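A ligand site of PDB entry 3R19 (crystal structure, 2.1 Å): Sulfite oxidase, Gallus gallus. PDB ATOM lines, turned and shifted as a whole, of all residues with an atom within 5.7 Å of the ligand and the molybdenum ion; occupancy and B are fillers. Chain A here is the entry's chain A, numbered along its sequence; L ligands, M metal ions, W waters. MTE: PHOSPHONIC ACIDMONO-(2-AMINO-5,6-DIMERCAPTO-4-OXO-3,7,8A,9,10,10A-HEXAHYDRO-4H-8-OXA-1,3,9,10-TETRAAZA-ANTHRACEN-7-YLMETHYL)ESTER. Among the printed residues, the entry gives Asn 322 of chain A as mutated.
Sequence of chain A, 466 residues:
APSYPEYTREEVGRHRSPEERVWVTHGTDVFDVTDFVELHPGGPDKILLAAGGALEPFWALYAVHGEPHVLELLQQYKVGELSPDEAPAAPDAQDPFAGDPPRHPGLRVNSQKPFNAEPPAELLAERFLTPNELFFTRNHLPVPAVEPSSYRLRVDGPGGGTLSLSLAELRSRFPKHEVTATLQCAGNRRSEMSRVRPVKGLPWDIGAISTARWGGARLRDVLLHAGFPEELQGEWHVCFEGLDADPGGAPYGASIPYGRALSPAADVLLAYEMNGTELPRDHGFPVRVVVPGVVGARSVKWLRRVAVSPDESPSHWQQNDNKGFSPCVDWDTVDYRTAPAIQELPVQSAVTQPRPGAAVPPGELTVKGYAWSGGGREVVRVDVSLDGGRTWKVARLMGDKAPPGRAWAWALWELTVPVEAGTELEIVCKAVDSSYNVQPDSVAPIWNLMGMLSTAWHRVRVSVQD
The backbone carbonyl oxygen (O) of Ser 299 sits at hydrogen-bond distance from a nitrogen (N8) of the ligand. An oxygen (O2P) of the ligand sits close to the backbone carbonyl oxygen (O) of Phe 136 (2.6 Å). N2 of the ligand is in hydrogen-bond range of O of Lys 301 (2.8 Å). O1P of the ligand lies within salt-bridge range of NZ of Lys 301, 2.8 Å away. A nitrogen (N5) of the ligand sits at hydrogen-bond distance from the backbone carbonyl oxygen (O) of Arg 138 (3.3 Å). An oxygen (O4) of the ligand is in hydrogen-bond range of a ring nitrogen (ND1) of His 140. An oxygen (O3P) of the ligand lies within salt-bridge range of the guanidinium group (NH1) of Arg 288. N2 of the ligand lies within hydrogen-bond range of OD1 of Asp 244, 2.8 Å away. N of Arg 138 lies within hydrogen-bond range of O1P of the ligand (3.0 Å). A ring nitrogen (ND1) of His 283 is in hydrogen-bond range of an oxygen (O3P) of the ligand (2.8 Å). The guanidinium group of Arg 138 lies close to a sulfur (S1') of the ligand (3.8 Å). The backbone NH (N) of His 140 is in hydrogen-bond range of an oxygen (O4) of the ligand. A nitrogen (N1) of the ligand lies within hydrogen-bond range of the backbone NH (N) of Lys 301, 2.8 Å away.
The guanidinium group (NH2) of Arg 288 lies within hydrogen-bond range of the backbone carbonyl oxygen (O) of Ser 299. The side-chain amino group (NZ) of Lys 301 is in hydrogen-bond range of the backbone carbonyl oxygen (O) of Asp 282 (3.1 Å). The backbone carbonyl oxygen of Asp 244 lies within hydrogen-bond range of the backbone NH of Tyr 252 (3.0 Å). The side-chain hydroxyl (OH) of Tyr 252 lies within hydrogen-bond range of the backbone carbonyl oxygen (O) of Ala 297, at 2.7 Å. The side-chain amino group (NZ) of Lys 301 lies within hydrogen-bond range of the backbone carbonyl oxygen (O) of Arg 138, 2.9 Å away. N of Gly 296 is in hydrogen-bond range of O of Gln 184 (2.9 Å). NE2 of His 140 is in hydrogen-bond range of NH2 of Arg 138, 3.4 Å away. The backbone carbonyl oxygen (O) of Trp 302 is in hydrogen-bond range of the backbone NH (N) of Leu 243, at 2.8 Å.
Residues that only touch the ligand: Gly 296 (3.2 Å), Tyr 252 (3.3 Å), Trp 302 (3.3 Å), Phe 135 (3.4 Å), Thr 137 (3.5 Å), Ala 297 (3.6 Å), Val 300 (3.6 Å), Asn 139 (3.9 Å), Gly 242 (3.9 Å) and Asp 282 (3.9 Å). Hydrophobic or aromatic side chains within 4 Å of the ligand: Phe 135, Phe 136, His 140, Tyr 252, His 283, Ala 297, Val 300 and Trp 302. 19 residues have an atom within 4 Å of the ligand: Phe 135, Phe 136, Thr 137, Arg 138, Asn 139, His 140, Cys 185, Gly 242, Asp 244, Tyr 252, Asp 282, His 283, Arg 288, Gly 296, Ala 297, Ser 299, Val 300, Lys 301 and Trp 302.
Ala 186 touches the molybdenum ion. Within 4 Å of the molybdenum ion: Cys 185 and Ala 186.
Water W2 binds the molybdenum ion (1.7 Å). The molybdenum ion is bound by water W1 (2.1 Å). The molybdenum ion is bound by S2' of the ligand (2.3 Å). A sulfur (S1') of the ligand binds the molybdenum ion (2.3 Å). SG of Cys 185 is bound to the molybdenum ion, at 2.5 Å.
Water W2 bridges N of Ala 186 (2.9 Å) and N of Ala 297 (3.4 Å).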
ATOM      1  N   PHE A 135       0.580  21.605  -9.135  1.00  0.00           N
ATOM      2  CA  PHE A 135      -0.036  20.931  -7.993  1.00  0.00           C
ATOM      3  C   PHE A 135       0.317  19.445  -8.068  1.00  0.00           C
ATOM      4  O   PHE A 135       0.121  18.805  -9.097  1.00  0.00           O
ATOM      5  CB  PHE A 135      -1.561  21.136  -8.048  1.00  0.00           C
ATOM      6  CG  PHE A 135      -2.255  20.951  -6.723  1.00  0.00           C
ATOM      7  CD1 PHE A 135      -2.469  19.669  -6.193  1.00  0.00           C
ATOM      8  CD2 PHE A 135      -2.754  22.060  -6.022  1.00  0.00           C
ATOM      9  CE1 PHE A 135      -3.148  19.507  -4.980  1.00  0.00           C
ATOM     10  CE2 PHE A 135      -3.431  21.907  -4.809  1.00  0.00           C
ATOM     11  CZ  PHE A 135      -3.627  20.610  -4.286  1.00  0.00           C
ATOM     12  N   PHE A 136       0.861  18.905  -6.974  1.00  0.00           N
ATOM     13  CA  PHE A 136       1.275  17.501  -6.958  1.00  0.00           C
ATOM     14  C   PHE A 136       0.116  16.603  -7.373  1.00  0.00           C
ATOM     15  O   PHE A 136      -1.045  16.912  -7.094  1.00  0.00           O
ATOM     16  CB  PHE A 136       1.849  17.069  -5.587  1.00  0.00           C
ATOM     17  CG  PHE A 136       0.820  16.547  -4.609  1.00  0.00           C
ATOM     18  CD1 PHE A 136       0.036  17.427  -3.855  1.00  0.00           C
ATOM     19  CD2 PHE A 136       0.637  15.169  -4.422  1.00  0.00           C
ATOM     20  CE1 PHE A 136      -0.926  16.947  -2.935  1.00  0.00           C
ATOM     21  CE2 PHE A 136      -0.307  14.686  -3.490  1.00  0.00           C
ATOM     22  CZ  PHE A 136      -1.085  15.584  -2.757  1.00  0.00           C
ATOM     23  N   THR A 137       0.449  15.505  -8.038  1.00  0.00           N
ATOM     24  CA  THR A 137      -0.572  14.592  -8.531  1.00  0.00           C
ATOM     25  C   THR A 137      -0.341  13.195  -7.978  1.00  0.00           C
ATOM     26  O   THR A 137       0.768  12.651  -8.065  1.00  0.00           O
ATOM     27  CB  THR A 137      -0.568  14.560 -10.067  1.00  0.00           C
ATOM     28  OG1 THR A 137      -0.812  15.880 -10.566  1.00  0.00           O
ATOM     29  CG2 THR A 137      -1.662  13.632 -10.595  1.00  0.00           C
ATOM     30  N   ARG A 138      -1.393  12.629  -7.401  1.00  0.00           N
ATOM     31  CA  ARG A 138      -1.333  11.281  -6.885  1.00  0.00           C
ATOM     32  C   ARG A 138      -2.531  10.509  -7.452  1.00  0.00           C
ATOM     33  O   ARG A 138      -3.678  10.719  -7.024  1.00  0.00           O
ATOM     34  CB  ARG A 138      -1.310  11.297  -5.346  1.00  0.00           C
ATOM     35  CG  ARG A 138      -0.762  10.038  -4.646  1.00  0.00           C
ATOM     36  CD  ARG A 138      -1.700   8.846  -4.742  1.00  0.00           C
ATOM     37  NE  ARG A 138      -1.186   7.679  -4.001  1.00  0.00           N
ATOM     38  CZ  ARG A 138      -0.698   6.580  -4.563  1.00  0.00           C
ATOM     39  NH1 ARG A 138      -0.629   6.470  -5.887  1.00  0.00           N
ATOM     40  NH2 ARG A 138      -0.269   5.588  -3.800  1.00  0.00           N
ATOM     41  N   ASN A 139      -2.259   9.637  -8.438  1.00  0.00           N
ATOM     42  CA  ASN A 139      -3.249   8.733  -9.020  1.00  0.00           C
ATOM     43  C   ASN A 139      -2.917   7.281  -8.686  1.00  0.00           C
ATOM     44  O   ASN A 139      -1.755   6.855  -8.827  1.00  0.00           O
ATOM     45  CB  ASN A 139      -3.290   8.865 -10.550  1.00  0.00           C
ATOM     46  CG  ASN A 139      -3.573  10.288 -11.029  1.00  0.00           C
ATOM     47  OD1 ASN A 139      -4.044  11.146 -10.268  1.00  0.00           O
ATOM     48  ND2 ASN A 139      -3.281  10.540 -12.299  1.00  0.00           N
ATOM     49  N   HIS A 140      -3.910   6.519  -8.242  1.00  0.00           N
ATOM     50  CA  HIS A 140      -3.728   5.064  -8.071  1.00  0.00           C
ATOM     51  C   HIS A 140      -3.926   4.298  -9.383  1.00  0.00           C
ATOM     52  O   HIS A 140      -3.456   3.161  -9.522  1.00  0.00           O
ATOM     53  CB  HIS A 140      -4.680   4.506  -7.014  1.00  0.00           C
ATOM     54  CG  HIS A 140      -4.351   4.937  -5.619  1.00  0.00           C
ATOM     55  ND1 HIS A 140      -4.736   6.154  -5.097  1.00  0.00           N
ATOM     56  CD2 HIS A 140      -3.676   4.299  -4.628  1.00  0.00           C
ATOM     57  CE1 HIS A 140      -4.305   6.254  -3.853  1.00  0.00           C
ATOM     58  NE2 HIS A 140      -3.666   5.140  -3.537  1.00  0.00           N
ATOM     59  N   LEU A 141      -4.630   4.924 -10.325  1.00  0.00           N
ATOM     60  CA  LEU A 141      -5.230   4.231 -11.453  1.00  0.00           C
ATOM     61  C   LEU A 141      -5.235   5.120 -12.699  1.00  0.00           C
ATOM     62  O   LEU A 141      -4.821   6.270 -12.621  1.00  0.00           O
ATOM     63  CB  LEU A 141      -6.673   3.808 -11.087  1.00  0.00           C
ATOM     64  CG  LEU A 141      -6.864   2.786  -9.949  1.00  0.00           C
ATOM     65  CD1 LEU A 141      -8.291   2.823  -9.371  1.00  0.00           C
ATOM     66  CD2 LEU A 141      -6.495   1.350 -10.398  1.00  0.00           C
ATOM     67  N   LEU A 183      -3.763  20.234   0.352  1.00  0.00           N
ATOM     68  CA  LEU A 183      -3.810  18.783   0.334  1.00  0.00           C
ATOM     69  C   LEU A 183      -2.403  18.264   0.540  1.00  0.00           C
ATOM     70  O   LEU A 183      -1.477  18.692  -0.138  1.00  0.00           O
ATOM     71  CB  LEU A 183      -4.389  18.271  -1.005  1.00  0.00           C
ATOM     72  CG  LEU A 183      -5.852  18.645  -1.307  1.00  0.00           C
ATOM     73  CD1 LEU A 183      -6.332  18.038  -2.622  1.00  0.00           C
ATOM     74  CD2 LEU A 183      -6.771  18.217  -0.155  1.00  0.00           C
ATOM     75  N   GLN A 184      -2.254  17.349   1.508  1.00  0.00           N
ATOM     76  CA  GLN A 184      -0.990  16.680   1.753  1.00  0.00           C
ATOM     77  C   GLN A 184      -1.202  15.187   1.744  1.00  0.00           C
ATOM     78  O   GLN A 184      -2.100  14.672   2.451  1.00  0.00           O
ATOM     79  CB  GLN A 184      -0.326  17.100   3.075  1.00  0.00           C
ATOM     80  CG  GLN A 184       1.011  16.371   3.279  1.00  0.00           C
ATOM     81  CD  GLN A 184       1.665  16.589   4.634  1.00  0.00           C
ATOM     82  OE1 GLN A 184       2.782  16.118   4.854  1.00  0.00           O
ATOM     83  NE2 GLN A 184       0.988  17.286   5.539  1.00  0.00           N
ATOM     84  N   CYS A 185      -0.391  14.495   0.960  1.00  0.00           N
ATOM     85  CA  CYS A 185      -0.455  13.047   0.910  1.00  0.00           C
ATOM     86  C   CYS A 185       0.129  12.444   2.182  1.00  0.00           C
ATOM     87  O   CYS A 185       1.051  13.014   2.771  1.00  0.00           O
ATOM     88  CB  CYS A 185       0.286  12.534  -0.335  1.00  0.00           C
ATOM     89  SG  CYS A 185       0.169  10.770  -0.599  1.00  0.00           S
ATOM     90  N   ALA A 186      -0.424  11.310   2.626  1.00  0.00           N
ATOM     91  CA  ALA A 186       0.089  10.575   3.791  1.00  0.00           C
ATOM     92  C   ALA A 186       1.561  10.187   3.622  1.00  0.00           C
ATOM     93  O   ALA A 186       2.323  10.094   4.603  1.00  0.00           O
ATOM     94  CB  ALA A 186      -0.742   9.311   4.019  1.00  0.00           C
ATOM     95  N   GLY A 187       1.956   9.962   2.381  1.00  0.00           N
ATOM     96  CA  GLY A 187       3.328   9.571   2.074  1.00  0.00           C
ATOM     97  C   GLY A 187       4.314  10.694   1.816  1.00  0.00           C
ATOM     98  O   GLY A 187       5.446  10.426   1.401  1.00  0.00           O
ATOM     99  N   TRP A 214     -10.329  26.148  -3.868  1.00  0.00           N
ATOM    100  CA  TRP A 214     -11.317  25.225  -4.408  1.00  0.00           C
ATOM    101  C   TRP A 214     -12.685  25.869  -4.389  1.00  0.00           C
ATOM    102  O   TRP A 214     -12.983  26.641  -3.478  1.00  0.00           O
ATOM    103  CB  TRP A 214     -11.363  23.960  -3.544  1.00  0.00           C
ATOM    104  CG  TRP A 214     -10.029  23.304  -3.345  1.00  0.00           C
ATOM    105  CD1 TRP A 214      -9.205  23.427  -2.272  1.00  0.00           C
ATOM    106  CD2 TRP A 214      -9.368  22.445  -4.271  1.00  0.00           C
ATOM    107  NE1 TRP A 214      -8.065  22.664  -2.463  1.00  0.00           N
ATOM    108  CE2 TRP A 214      -8.145  22.049  -3.675  1.00  0.00           C
ATOM    109  CE3 TRP A 214      -9.693  21.947  -5.540  1.00  0.00           C
ATOM    110  CZ2 TRP A 214      -7.244  21.188  -4.310  1.00  0.00           C
ATOM    111  CZ3 TRP A 214      -8.789  21.096  -6.176  1.00  0.00           C
ATOM    112  CH2 TRP A 214      -7.593  20.729  -5.554  1.00  0.00           C
ATOM    113  N   GLY A 242     -14.808   6.816  -6.534  1.00  0.00           N
ATOM    114  CA  GLY A 242     -14.339   7.450  -7.755  1.00  0.00           C
ATOM    115  C   GLY A 242     -14.754   6.667  -8.993  1.00  0.00           C
ATOM    116  O   GLY A 242     -15.128   5.494  -8.905  1.00  0.00           O
ATOM    117  N   LEU A 243     -14.689   7.317 -10.147  1.00  0.00           N
ATOM    118  CA  LEU A 243     -14.915   6.661 -11.438  1.00  0.00           C
ATOM    119  C   LEU A 243     -13.742   5.766 -11.869  1.00  0.00           C
ATOM    120  O   LEU A 243     -13.911   4.911 -12.731  1.00  0.00           O
ATOM    121  CB  LEU A 243     -15.195   7.715 -12.536  1.00  0.00           C
ATOM    122  CG  LEU A 243     -16.591   8.341 -12.587  1.00  0.00           C
ATOM    123  CD1 LEU A 243     -16.558   9.600 -13.442  1.00  0.00           C
ATOM    124  CD2 LEU A 243     -17.648   7.353 -13.109  1.00  0.00           C
ATOM    125  N   ASP A 244     -12.566   5.968 -11.266  1.00  0.00           N
ATOM    126  CA  ASP A 244     -11.407   5.114 -11.560  1.00  0.00           C
ATOM    127  C   ASP A 244     -11.529   3.767 -10.857  1.00  0.00           C
ATOM    128  O   ASP A 244     -11.852   3.704  -9.672  1.00  0.00           O
ATOM    129  CB  ASP A 244     -10.078   5.823 -11.230  1.00  0.00           C
ATOM    130  CG  ASP A 244     -10.006   6.357  -9.802  1.00  0.00           C
ATOM    131  OD1 ASP A 244     -11.059   6.756  -9.248  1.00  0.00           O
ATOM    132  OD2 ASP A 244      -8.875   6.434  -9.254  1.00  0.00           O
ATOM    133  N   TYR A 252     -11.748   3.338  -6.674  1.00  0.00           N
ATOM    134  CA  TYR A 252     -11.106   4.019  -5.572  1.00  0.00           C
ATOM    135  C   TYR A 252     -12.184   4.515  -4.625  1.00  0.00           C
ATOM    136  O   TYR A 252     -13.186   5.082  -5.064  1.00  0.00           O
ATOM    137  CB  TYR A 252     -10.221   5.209  -6.003  1.00  0.00           C
ATOM    138  CG  TYR A 252      -9.485   5.801  -4.807  1.00  0.00           C
ATOM    139  CD1 TYR A 252      -8.338   5.184  -4.283  1.00  0.00           C
ATOM    140  CD2 TYR A 252      -9.987   6.929  -4.148  1.00  0.00           C
ATOM    141  CE1 TYR A 252      -7.682   5.720  -3.151  1.00  0.00           C
ATOM    142  CE2 TYR A 252      -9.341   7.456  -3.035  1.00  0.00           C
ATOM    143  CZ  TYR A 252      -8.197   6.858  -2.543  1.00  0.00           C
ATOM    144  OH  TYR A 252      -7.577   7.401  -1.444  1.00  0.00           O
ATOM    145  N   ASP A 282      -6.370  15.422 -14.174  1.00  0.00           N
ATOM    146  CA  ASP A 282      -5.500  14.843 -13.142  1.00  0.00           C
ATOM    147  C   ASP A 282      -5.965  15.154 -11.711  1.00  0.00           C
ATOM    148  O   ASP A 282      -5.597  14.464 -10.762  1.00  0.00           O
ATOM    149  CB  ASP A 282      -4.059  15.336 -13.321  1.00  0.00           C
ATOM    150  CG  ASP A 282      -3.171  14.359 -14.091  1.00  0.00           C
ATOM    151  OD1 ASP A 282      -3.495  13.145 -14.197  1.00  0.00           O
ATOM    152  OD2 ASP A 282      -2.116  14.795 -14.589  1.00  0.00           O
ATOM    153  N   HIS A 283      -6.764  16.215 -11.564  1.00  0.00           N
ATOM    154  CA  HIS A 283      -7.205  16.628 -10.249  1.00  0.00           C
ATOM    155  C   HIS A 283      -8.681  16.373  -9.987  1.00  0.00           C
ATOM    156  O   HIS A 283      -9.258  16.854  -9.019  1.00  0.00           O
ATOM    157  CB  HIS A 283      -6.752  18.067  -9.966  1.00  0.00           C
ATOM    158  CG  HIS A 283      -5.262  18.217  -9.988  1.00  0.00           C
ATOM    159  ND1 HIS A 283      -4.455  17.703  -8.995  1.00  0.00           N
ATOM    160  CD2 HIS A 283      -4.430  18.759 -10.903  1.00  0.00           C
ATOM    161  CE1 HIS A 283      -3.185  17.943  -9.292  1.00  0.00           C
ATOM    162  NE2 HIS A 283      -3.144  18.578 -10.447  1.00  0.00           N
ATOM    163  N   ARG A 288     -14.525  16.567  -7.569  1.00  0.00           N
ATOM    164  CA  ARG A 288     -13.813  15.851  -6.510  1.00  0.00           C
ATOM    165  C   ARG A 288     -14.370  16.274  -5.145  1.00  0.00           C
ATOM    166  O   ARG A 288     -14.953  17.365  -5.012  1.00  0.00           O
ATOM    167  CB  ARG A 288     -12.297  16.137  -6.569  1.00  0.00           C
ATOM    168  CG  ARG A 288     -11.884  17.487  -5.982  1.00  0.00           C
ATOM    169  CD  ARG A 288     -10.369  17.657  -5.883  1.00  0.00           C
ATOM    170  NE  ARG A 288      -9.733  16.598  -5.079  1.00  0.00           N
ATOM    171  CZ  ARG A 288      -8.429  16.338  -5.119  1.00  0.00           C
ATOM    172  NH1 ARG A 288      -7.639  17.060  -5.908  1.00  0.00           N
ATOM    173  NH2 ARG A 288      -7.914  15.346  -4.389  1.00  0.00           N
ATOM    174  N   VAL A 295      -6.017  14.220   5.457  1.00  0.00           N
ATOM    175  CA  VAL A 295      -5.075  13.611   4.476  1.00  0.00           C
ATOM    176  C   VAL A 295      -5.684  13.565   3.064  1.00  0.00           C
ATOM    177  O   VAL A 295      -6.891  13.411   2.908  1.00  0.00           O
ATOM    178  CB  VAL A 295      -4.608  12.174   4.940  1.00  0.00           C
ATOM    179  CG1 VAL A 295      -5.785  11.193   5.052  1.00  0.00           C
ATOM    180  CG2 VAL A 295      -3.544  11.632   4.025  1.00  0.00           C
ATOM    181  N   GLY A 296      -4.829  13.726   2.055  1.00  0.00           N
ATOM    182  CA  GLY A 296      -5.282  13.777   0.649  1.00  0.00           C
ATOM    183  C   GLY A 296      -6.125  12.588   0.208  1.00  0.00           C
ATOM    184  O   GLY A 296      -7.050  12.758  -0.601  1.00  0.00           O
ATOM    185  N   ALA A 297      -5.808  11.404   0.704  1.00  0.00           N
ATOM    186  CA  ALA A 297      -6.555  10.158   0.415  1.00  0.00           C
ATOM    187  C   ALA A 297      -8.089  10.236   0.469  1.00  0.00           C
ATOM    188  O   ALA A 297      -8.761   9.487  -0.259  1.00  0.00           O
ATOM    189  CB  ALA A 297      -6.064   9.005   1.325  1.00  0.00           C
ATOM    190  N   ARG A 298      -8.620  11.092   1.325  1.00  0.00           N
ATOM    191  CA  ARG A 298     -10.074  11.179   1.536  1.00  0.00           C
ATOM    192  C   ARG A 298     -10.726  12.130   0.526  1.00  0.00           C
ATOM    193  O   ARG A 298     -11.937  12.067   0.314  1.00  0.00           O
ATOM    194  CB  ARG A 298     -10.428  11.619   2.976  1.00  0.00           C
ATOM    195  CG  ARG A 298      -9.725  10.848   4.119  1.00  0.00           C
ATOM    196  CD  ARG A 298      -9.800   9.328   4.002  1.00  0.00           C
ATOM    197  NE  ARG A 298      -8.788   8.707   4.858  1.00  0.00           N
ATOM    198  CZ  ARG A 298      -8.150   7.576   4.601  1.00  0.00           C
ATOM    199  NH1 ARG A 298      -8.442   6.853   3.510  1.00  0.00           N
ATOM    200  NH2 ARG A 298      -7.219   7.138   5.448  1.00  0.00           N
ATOM    201  N   SER A 299      -9.921  12.989  -0.100  1.00  0.00           N
ATOM    202  CA  SER A 299     -10.435  13.906  -1.126  1.00  0.00           C
ATOM    203  C   SER A 299     -10.620  13.187  -2.461  1.00  0.00           C
ATOM    204  O   SER A 299      -9.831  13.357  -3.405  1.00  0.00           O
ATOM    205  CB  SER A 299      -9.527  15.134  -1.276  1.00  0.00           C
ATOM    206  OG  SER A 299      -9.631  15.954  -0.122  1.00  0.00           O
ATOM    207  N   VAL A 300     -11.659  12.371  -2.529  1.00  0.00           N
ATOM    208  CA  VAL A 300     -11.868  11.492  -3.674  1.00  0.00           C
ATOM    209  C   VAL A 300     -12.104  12.246  -4.990  1.00  0.00           C
ATOM    210  O   VAL A 300     -13.017  13.065  -5.096  1.00  0.00           O
ATOM    211  CB  VAL A 300     -13.010  10.499  -3.418  1.00  0.00           C
ATOM    212  CG1 VAL A 300     -13.269   9.638  -4.648  1.00  0.00           C
ATOM    213  CG2 VAL A 300     -12.653   9.597  -2.214  1.00  0.00           C
ATOM    214  N   LYS A 301     -11.276  11.941  -5.989  1.00  0.00           N
ATOM    215  CA  LYS A 301     -11.378  12.562  -7.305  1.00  0.00           C
ATOM    216  C   LYS A 301     -12.335  11.799  -8.215  1.00  0.00           C
ATOM    217  O   LYS A 301     -12.643  10.618  -7.971  1.00  0.00           O
ATOM    218  CB  LYS A 301      -9.991  12.635  -7.944  1.00  0.00           C
ATOM    219  CG  LYS A 301      -9.021  13.590  -7.246  1.00  0.00           C
ATOM    220  CD  LYS A 301      -7.667  13.667  -7.958  1.00  0.00           C
ATOM    221  CE  LYS A 301      -6.807  12.416  -7.696  1.00  0.00           C
ATOM    222  NZ  LYS A 301      -5.480  12.522  -8.382  1.00  0.00           N
ATOM    223  N   TRP A 302     -12.811  12.469  -9.273  1.00  0.00           N
ATOM    224  CA  TRP A 302     -13.693  11.858 -10.278  1.00  0.00           C
ATOM    225  C   TRP A 302     -14.900  11.199  -9.606  1.00  0.00           C
ATOM    226  O   TRP A 302     -15.232  10.050  -9.898  1.00  0.00           O
ATOM    227  CB  TRP A 302     -12.918  10.841 -11.154  1.00  0.00           C
ATOM    228  CG  TRP A 302     -11.602  11.380 -11.648  1.00  0.00           C
ATOM    229  CD1 TRP A 302     -11.410  12.349 -12.602  1.00  0.00           C
ATOM    230  CD2 TRP A 302     -10.302  10.979 -11.227  1.00  0.00           C
ATOM    231  NE1 TRP A 302     -10.071  12.579 -12.782  1.00  0.00           N
ATOM    232  CE2 TRP A 302      -9.363  11.751 -11.947  1.00  0.00           C
ATOM    233  CE3 TRP A 302      -9.828  10.025 -10.302  1.00  0.00           C
ATOM    234  CZ2 TRP A 302      -7.978  11.616 -11.768  1.00  0.00           C
ATOM    235  CZ3 TRP A 302      -8.462   9.895 -10.124  1.00  0.00           C
ATOM    236  CH2 TRP A 302      -7.550  10.683 -10.858  1.00  0.00           C
ATOM    237  N   ASN A 322      -2.755   3.812   4.253  1.00  0.00           N
ATOM    238  CA  ASN A 322      -2.858   5.102   4.914  1.00  0.00           C
ATOM    239  C   ASN A 322      -3.246   4.966   6.390  1.00  0.00           C
ATOM    240  O   ASN A 322      -4.264   5.517   6.846  1.00  0.00           O
ATOM    241  CB  ASN A 322      -3.804   6.041   4.143  1.00  0.00           C
ATOM    242  CG  ASN A 322      -3.298   6.307   2.728  1.00  0.00           C
ATOM    243  OD1 ASN A 322      -2.140   6.681   2.524  1.00  0.00           O
ATOM    244  ND2 ASN A 322      -4.164   6.085   1.749  1.00  0.00           N
HETATM  245  N1  MTE L   1      -9.363   9.912  -5.804  1.00  0.00           N
HETATM  246  C2  MTE L   1      -9.464   8.926  -6.722  1.00  0.00           C
HETATM  247  N2  MTE L   1     -10.658   8.727  -7.336  1.00  0.00           N
HETATM  248  N3  MTE L   1      -8.432   8.131  -7.049  1.00  0.00           N
HETATM  249  C4  MTE L   1      -7.216   8.270  -6.489  1.00  0.00           C
HETATM  250  O4  MTE L   1      -6.296   7.522  -6.819  1.00  0.00           O
HETATM  251  N5  MTE L   1      -5.837   9.567  -4.797  1.00  0.00           N
HETATM  252  C6  MTE L   1      -6.012  10.084  -3.427  1.00  0.00           C
HETATM  253  C7  MTE L   1      -6.882  11.338  -3.469  1.00  0.00           C
HETATM  254  N8  MTE L   1      -8.122  11.143  -4.238  1.00  0.00           N
HETATM  255  C9  MTE L   1      -7.015   9.331  -5.458  1.00  0.00           C
HETATM  256  C10 MTE L   1      -8.202  10.161  -5.155  1.00  0.00           C
HETATM  257  C1' MTE L   1      -4.729  10.401  -2.693  1.00  0.00           C
HETATM  258  S1' MTE L   1      -3.935   9.141  -1.873  1.00  0.00           S
HETATM  259  C2' MTE L   1      -4.264  11.661  -2.659  1.00  0.00           C
HETATM  260  S2' MTE L   1      -2.845  12.045  -1.788  1.00  0.00           S
HETATM  261  C3' MTE L   1      -4.995  12.799  -3.365  1.00  0.00           C
HETATM  262  O3' MTE L   1      -6.122  12.341  -4.128  1.00  0.00           O
HETATM  263  C4' MTE L   1      -4.086  13.567  -4.319  1.00  0.00           C
HETATM  264  O4' MTE L   1      -4.799  14.632  -4.959  1.00  0.00           O
HETATM  265  P   MTE L   1      -4.154  15.439  -6.198  1.00  0.00           P
HETATM  266  O1P MTE L   1      -3.786  14.416  -7.257  1.00  0.00           O
HETATM  267  O2P MTE L   1      -3.002  16.144  -5.520  1.00  0.00           O
HETATM  268  O3P MTE L   1      -5.260  16.336  -6.687  1.00  0.00           O
HETATM  269 MO    MO M   1      -2.204  10.115  -0.664  1.00  0.00          MO
HETATM  270  O   HOH W   1      -1.315   8.223  -0.981  1.00  0.00           O
HETATM  271  O   HOH W   2      -2.597  10.419   0.964  1.00  0.00           O
